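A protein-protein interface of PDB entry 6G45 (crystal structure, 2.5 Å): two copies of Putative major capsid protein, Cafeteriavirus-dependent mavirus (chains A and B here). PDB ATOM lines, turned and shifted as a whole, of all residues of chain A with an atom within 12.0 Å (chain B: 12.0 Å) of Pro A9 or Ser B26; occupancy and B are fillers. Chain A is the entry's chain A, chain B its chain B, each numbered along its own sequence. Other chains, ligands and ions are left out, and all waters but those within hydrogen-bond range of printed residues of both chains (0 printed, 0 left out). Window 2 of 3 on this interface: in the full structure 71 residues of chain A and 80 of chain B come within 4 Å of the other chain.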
ATOM      1  N   ASN A   6     -28.768   8.688  -1.703  1.00  0.00           N
ATOM      2  CA  ASN A   6     -27.972   7.536  -2.244  1.00  0.00           C
ATOM      3  C   ASN A   6     -26.646   8.004  -2.836  1.00  0.00           C
ATOM      4  O   ASN A   6     -26.617   8.939  -3.635  1.00  0.00           O
ATOM      5  CB  ASN A   6     -28.756   6.769  -3.318  1.00  0.00           C
ATOM      6  CG  ASN A   6     -29.945   6.019  -2.754  1.00  0.00           C
ATOM      7  OD1 ASN A   6     -29.806   5.214  -1.837  1.00  0.00           O
ATOM      8  ND2 ASN A   6     -31.121   6.271  -3.311  1.00  0.00           N
ATOM      9  N   THR A   7     -25.561   7.339  -2.444  1.00  0.00           N
ATOM     10  CA  THR A   7     -24.223   7.642  -2.951  1.00  0.00           C
ATOM     11  C   THR A   7     -23.397   6.342  -3.028  1.00  0.00           C
ATOM     12  O   THR A   7     -23.523   5.488  -2.142  1.00  0.00           O
ATOM     13  CB  THR A   7     -23.523   8.715  -2.075  1.00  0.00           C
ATOM     14  OG1 THR A   7     -22.251   9.048  -2.643  1.00  0.00           O
ATOM     15  CG2 THR A   7     -23.334   8.246  -0.621  1.00  0.00           C
ATOM     16  N   PRO A   8     -22.567   6.173  -4.087  1.00  0.00           N
ATOM     17  CA  PRO A   8     -21.736   4.961  -4.167  1.00  0.00           C
ATOM     18  C   PRO A   8     -20.723   4.847  -3.020  1.00  0.00           C
ATOM     19  O   PRO A   8     -20.089   5.846  -2.677  1.00  0.00           O
ATOM     20  CB  PRO A   8     -20.997   5.117  -5.503  1.00  0.00           C
ATOM     21  CG  PRO A   8     -21.826   6.057  -6.297  1.00  0.00           C
ATOM     22  CD  PRO A   8     -22.442   6.996  -5.306  1.00  0.00           C
ATOM     23  N   PRO A   9     -20.572   3.642  -2.434  1.00  0.00           N
ATOM     24  CA  PRO A   9     -19.645   3.465  -1.311  1.00  0.00           C
ATOM     25  C   PRO A   9     -18.178   3.470  -1.739  1.00  0.00           C
ATOM     26  O   PRO A   9     -17.869   3.125  -2.881  1.00  0.00           O
ATOM     27  CB  PRO A   9     -20.035   2.093  -0.754  1.00  0.00           C
ATOM     28  CG  PRO A   9     -20.548   1.350  -1.936  1.00  0.00           C
ATOM     29  CD  PRO A   9     -21.229   2.373  -2.804  1.00  0.00           C
ATOM     30  N   GLU A  10     -17.293   3.864  -0.822  1.00  0.00           N
ATOM     31  CA  GLU A  10     -15.852   3.829  -1.061  1.00  0.00           C
ATOM     32  C   GLU A  10     -15.392   2.380  -1.154  1.00  0.00           C
ATOM     33  O   GLU A  10     -15.813   1.539  -0.355  1.00  0.00           O
ATOM     34  CB  GLU A  10     -15.086   4.507   0.077  1.00  0.00           C
ATOM     35  CG  GLU A  10     -15.486   5.948   0.358  1.00  0.00           C
ATOM     36  CD  GLU A  10     -14.585   6.619   1.390  1.00  0.00           C
ATOM     37  OE1 GLU A  10     -14.089   5.928   2.308  1.00  0.00           O
ATOM     38  OE2 GLU A  10     -14.374   7.847   1.285  1.00  0.00           O
ATOM     39  N   LEU A  11     -14.533   2.101  -2.132  1.00  0.00           N
ATOM     40  CA  LEU A  11     -13.963   0.772  -2.326  1.00  0.00           C
ATOM     41  C   LEU A  11     -12.453   0.842  -2.131  1.00  0.00           C
ATOM     42  O   LEU A  11     -11.803   1.778  -2.605  1.00  0.00           O
ATOM     43  CB  LEU A  11     -14.294   0.247  -3.724  1.00  0.00           C
ATOM     44  CG  LEU A  11     -15.779   0.172  -4.090  1.00  0.00           C
ATOM     45  CD1 LEU A  11     -15.958  -0.136  -5.567  1.00  0.00           C
ATOM     46  CD2 LEU A  11     -16.486  -0.870  -3.241  1.00  0.00           C
ATOM     47  N   ASP A  12     -11.906  -0.143  -1.422  1.00  0.00           N
ATOM     48  CA  ASP A  12     -10.462  -0.268  -1.248  1.00  0.00           C
ATOM     49  C   ASP A  12      -9.795  -0.620  -2.573  1.00  0.00           C
ATOM     50  O   ASP A  12     -10.409  -1.237  -3.451  1.00  0.00           O
ATOM     51  CB  ASP A  12     -10.131  -1.345  -0.205  1.00  0.00           C
ATOM     52  CG  ASP A  12     -10.587  -0.974   1.202  1.00  0.00           C
ATOM     53  OD1 ASP A  12     -10.727   0.231   1.513  1.00  0.00           O
ATOM     54  OD2 ASP A  12     -10.792  -1.903   2.010  1.00  0.00           O
ATOM     55  N   THR A  13      -8.534  -0.215  -2.701  1.00  0.00           N
ATOM     56  CA  THR A  13      -7.749  -0.435  -3.912  1.00  0.00           C
ATOM     57  C   THR A  13      -6.586  -1.389  -3.645  1.00  0.00           C
ATOM     58  O   THR A  13      -6.083  -1.469  -2.521  1.00  0.00           O
ATOM     59  CB  THR A  13      -7.201   0.895  -4.465  1.00  0.00           C
ATOM     60  OG1 THR A  13      -6.486   1.591  -3.435  1.00  0.00           O
ATOM     61  CG2 THR A  13      -8.339   1.771  -4.965  1.00  0.00           C
ATOM     62  N   VAL A  14      -6.181  -2.115  -4.687  1.00  0.00           N
ATOM     63  CA  VAL A  14      -5.001  -2.984  -4.645  1.00  0.00           C
ATOM     64  C   VAL A  14      -4.131  -2.733  -5.874  1.00  0.00           C
ATOM     65  O   VAL A  14      -4.642  -2.427  -6.954  1.00  0.00           O
ATOM     66  CB  VAL A  14      -5.374  -4.487  -4.559  1.00  0.00           C
ATOM     67  CG1 VAL A  14      -6.135  -4.770  -3.272  1.00  0.00           C
ATOM     68  CG2 VAL A  14      -6.186  -4.945  -5.768  1.00  0.00           C
ATOM     69  N   ASN B  22     -23.452 -14.858  -3.562  1.00  0.00           N
ATOM     70  CA  ASN B  22     -22.331 -14.151  -2.944  1.00  0.00           C
ATOM     71  C   ASN B  22     -22.322 -12.718  -3.486  1.00  0.00           C
ATOM     72  O   ASN B  22     -21.605 -12.396  -4.440  1.00  0.00           O
ATOM     73  CB  ASN B  22     -21.001 -14.870  -3.213  1.00  0.00           C
ATOM     74  CG  ASN B  22     -19.840 -14.262  -2.438  1.00  0.00           C
ATOM     75  OD1 ASN B  22     -20.003 -13.805  -1.303  1.00  0.00           O
ATOM     76  ND2 ASN B  22     -18.659 -14.258  -3.051  1.00  0.00           N
ATOM     77  N   TRP B  23     -23.136 -11.872  -2.858  1.00  0.00           N
ATOM     78  CA  TRP B  23     -23.441 -10.539  -3.376  1.00  0.00           C
ATOM     79  C   TRP B  23     -22.186  -9.675  -3.340  1.00  0.00           C
ATOM     80  O   TRP B  23     -21.563  -9.558  -2.283  1.00  0.00           O
ATOM     81  CB  TRP B  23     -24.545  -9.867  -2.550  1.00  0.00           C
ATOM     82  CG  TRP B  23     -25.813 -10.660  -2.437  1.00  0.00           C
ATOM     83  CD1 TRP B  23     -26.212 -11.409  -1.369  1.00  0.00           C
ATOM     84  CD2 TRP B  23     -26.847 -10.787  -3.422  1.00  0.00           C
ATOM     85  NE1 TRP B  23     -27.426 -11.998  -1.625  1.00  0.00           N
ATOM     86  CE2 TRP B  23     -27.841 -11.632  -2.877  1.00  0.00           C
ATOM     87  CE3 TRP B  23     -27.034 -10.269  -4.711  1.00  0.00           C
ATOM     88  CZ2 TRP B  23     -29.005 -11.972  -3.575  1.00  0.00           C
ATOM     89  CZ3 TRP B  23     -28.198 -10.609  -5.408  1.00  0.00           C
ATOM     90  CH2 TRP B  23     -29.164 -11.453  -4.835  1.00  0.00           C
ATOM     91  N   PRO B  24     -21.786  -9.096  -4.492  1.00  0.00           N
ATOM     92  CA  PRO B  24     -20.678  -8.140  -4.437  1.00  0.00           C
ATOM     93  C   PRO B  24     -21.110  -6.839  -3.755  1.00  0.00           C
ATOM     94  O   PRO B  24     -22.101  -6.227  -4.161  1.00  0.00           O
ATOM     95  CB  PRO B  24     -20.318  -7.912  -5.914  1.00  0.00           C
ATOM     96  CG  PRO B  24     -20.989  -8.999  -6.675  1.00  0.00           C
ATOM     97  CD  PRO B  24     -22.194  -9.379  -5.880  1.00  0.00           C
ATOM     98  N   THR B  25     -20.378  -6.456  -2.711  1.00  0.00           N
ATOM     99  CA  THR B  25     -20.642  -5.249  -1.926  1.00  0.00           C
ATOM    100  C   THR B  25     -19.307  -4.553  -1.668  1.00  0.00           C
ATOM    101  O   THR B  25     -18.261  -5.024  -2.117  1.00  0.00           O
ATOM    102  CB  THR B  25     -21.319  -5.585  -0.574  1.00  0.00           C
ATOM    103  OG1 THR B  25     -20.411  -6.315   0.260  1.00  0.00           O
ATOM    104  CG2 THR B  25     -22.585  -6.413  -0.776  1.00  0.00           C
ATOM    105  N   SER B  26     -19.341  -3.441  -0.938  1.00  0.00           N
ATOM    106  CA  SER B  26     -18.116  -2.754  -0.520  1.00  0.00           C
ATOM    107  C   SER B  26     -17.224  -3.574   0.432  1.00  0.00           C
ATOM    108  O   SER B  26     -16.037  -3.285   0.563  1.00  0.00           O
ATOM    109  CB  SER B  26     -18.455  -1.398   0.110  1.00  0.00           C
ATOM    110  OG  SER B  26     -19.195  -1.549   1.308  1.00  0.00           O
ATOM    111  N   LYS B  27     -17.800  -4.580   1.093  1.00  0.00           N
ATOM    112  CA  LYS B  27     -17.061  -5.474   1.987  1.00  0.00           C
ATOM    113  C   LYS B  27     -16.194  -6.530   1.284  1.00  0.00           C
ATOM    114  O   LYS B  27     -15.255  -7.042   1.896  1.00  0.00           O
ATOM    115  CB  LYS B  27     -18.037  -6.169   2.944  1.00  0.00           C
ATOM    116  CG  LYS B  27     -18.811  -5.199   3.824  1.00  0.00           C
ATOM    117  CD  LYS B  27     -19.688  -5.917   4.837  1.00  0.00           C
ATOM    118  CE  LYS B  27     -20.475  -4.918   5.676  1.00  0.00           C
ATOM    119  NZ  LYS B  27     -21.248  -5.576   6.766  1.00  0.00           N
ATOM    120  N   ASN B  28     -16.506  -6.865   0.030  1.00  0.00           N
ATOM    121  CA  ASN B  28     -15.780  -7.926  -0.703  1.00  0.00           C
ATOM    122  C   ASN B  28     -15.336  -7.595  -2.144  1.00  0.00           C
ATOM    123  O   ASN B  28     -14.847  -8.481  -2.844  1.00  0.00           O
ATOM    124  CB  ASN B  28     -16.607  -9.230  -0.682  1.00  0.00           C
ATOM    125  CG  ASN B  28     -17.962  -9.090  -1.364  1.00  0.00           C
ATOM    126  OD1 ASN B  28     -18.308  -8.030  -1.886  1.00  0.00           O
ATOM    127  ND2 ASN B  28     -18.735 -10.168  -1.363  1.00  0.00           N
ATOM    128  N   VAL B  29     -15.489  -6.342  -2.575  1.00  0.00           N
ATOM    129  CA  VAL B  29     -15.083  -5.905  -3.918  1.00  0.00           C
ATOM    130  C   VAL B  29     -13.979  -4.863  -3.791  1.00  0.00           C
ATOM    131  O   VAL B  29     -14.142  -3.869  -3.086  1.00  0.00           O
ATOM    132  CB  VAL B  29     -16.261  -5.292  -4.712  1.00  0.00           C
ATOM    133  CG1 VAL B  29     -15.793  -4.691  -6.033  1.00  0.00           C
ATOM    134  CG2 VAL B  29     -17.329  -6.340  -4.972  1.00  0.00           C
ATOM    135  N   LYS B  30     -12.868  -5.099  -4.487  1.00  0.00           N
ATOM    136  CA  LYS B  30     -11.746  -4.167  -4.531  1.00  0.00           C
ATOM    137  C   LYS B  30     -11.415  -3.815  -5.978  1.00  0.00           C
ATOM    138  O   LYS B  30     -11.636  -4.620  -6.885  1.00  0.00           O
ATOM    139  CB  LYS B  30     -10.533  -4.772  -3.822  1.00  0.00           C
ATOM    140  CG  LYS B  30     -10.730  -4.912  -2.320  1.00  0.00           C
ATOM    141  CD  LYS B  30      -9.553  -5.596  -1.644  1.00  0.00           C
ATOM    142  CE  LYS B  30      -9.797  -5.738  -0.150  1.00  0.00           C
ATOM    143  NZ  LYS B  30      -8.679  -6.432   0.547  1.00  0.00           N
ATOM    144  N   ILE B  31     -10.897  -2.604  -6.179  1.00  0.00           N
ATOM    145  CA  ILE B  31     -10.541  -2.102  -7.506  1.00  0.00           C
ATOM    146  C   ILE B  31      -9.036  -2.223  -7.709  1.00  0.00           C
ATOM    147  O   ILE B  31      -8.252  -1.679  -6.930  1.00  0.00           O
ATOM    148  CB  ILE B  31     -10.964  -0.628  -7.692  1.00  0.00           C
ATOM    149  CG1 ILE B  31     -12.451  -0.435  -7.358  1.00  0.00           C
ATOM    150  CG2 ILE B  31     -10.684  -0.149  -9.114  1.00  0.00           C
ATOM    151  CD1 ILE B  31     -13.410  -1.308  -8.147  1.00  0.00           C
ATOM    152  N   ALA B  32      -8.649  -2.931  -8.766  1.00  0.00           N
ATOM    153  CA  ALA B  32      -7.248  -3.154  -9.091  1.00  0.00           C
ATOM    154  C   ALA B  32      -6.753  -2.132 -10.106  1.00  0.00           C
ATOM    155  O   ALA B  32      -7.411  -1.874 -11.114  1.00  0.00           O
ATOM    156  CB  ALA B  32      -7.059  -4.559  -9.641  1.00  0.00           C
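O of Asp A12 sits at hydrogen-bond distance from N of Ile B31.
The backbone carbonyl oxygen (O) of Ile B31 sits at hydrogen-bond distance from the backbone NH (N) of Val A14 (3.1 Å).
Among the printed residues, merely in contact across the chains: Pro A9 with Ser B26 (3.9 Å), Glu A10 with Ser B26 (3.98 Å), Leu A11 with Ser B26 (3.7 Å), Leu A11 with Val B29 (3.8 Å), Leu A11 with Ile B31 (3.8 Å), Asp A12 with Lys B30 (3.4 Å), Thr A13 with Ile B31 (3.3 Å), Val A14 with Lys B30 (3.9 Å) and Val A14 with Ala B32 (3.4 Å).
No residue of chain B comes within 4 Å of Thr A7.
No residue of chain B comes within 4 Å of Pro A8.
Of chain B, only Ser B26 (3.9 Å) comes within 4 Å of Pro A9.
Glu A10 touches just one residue of chain B: Ser B26.
Of the printed residues of chain B, Val A14 touches Lys B30 (3.9 Å), Ile B31 (3.1 Å) and Ala B32 (3.4 Å).
Pro B24 touches none of the printed residues of chain A.
Ser B26 touches just these residues of chain A: Pro A9, Glu A10 and Leu A11.
Lys B27 touches none of the printed residues of chain A.
No residue of chain A comes within 4 Å of Asn B28.
Of chain A, only Leu A11 (3.8 Å) comes within 4 Å of Val B29.
Of the printed residues of chain A, Lys B30 touches Asp A12 and Val A14.
Of the printed residues of chain A, Ile B31 touches Leu A11 (3.8 Å), Asp A12 (3.1 Å), Thr A13 (3.3 Å) and Val A14 (3.1 Å).
Of the printed residues of chain A, Ala B32 touches Val A14 (3.4 Å).
The nearest residue of chain A that does not touch Ser B26 is Asp A12 (5.6 Å).
Of the 11 printed residues of chain B, 5 touch a printed residue of chain A.
Hydrophobic or aromatic side chains of chain B within 4 Å of the printed part of chain A: Ile B31 and Ala B32.
Of the 9 printed residues of chain A, 6 touch a printed residue of chain B.
Among the printed residues, 11 pairs touch across the chains.
No position is printed for both chains.
Of the 11 pairs that touch across the chains among the printed residues, none has its exchanged pair printed and touching as well.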
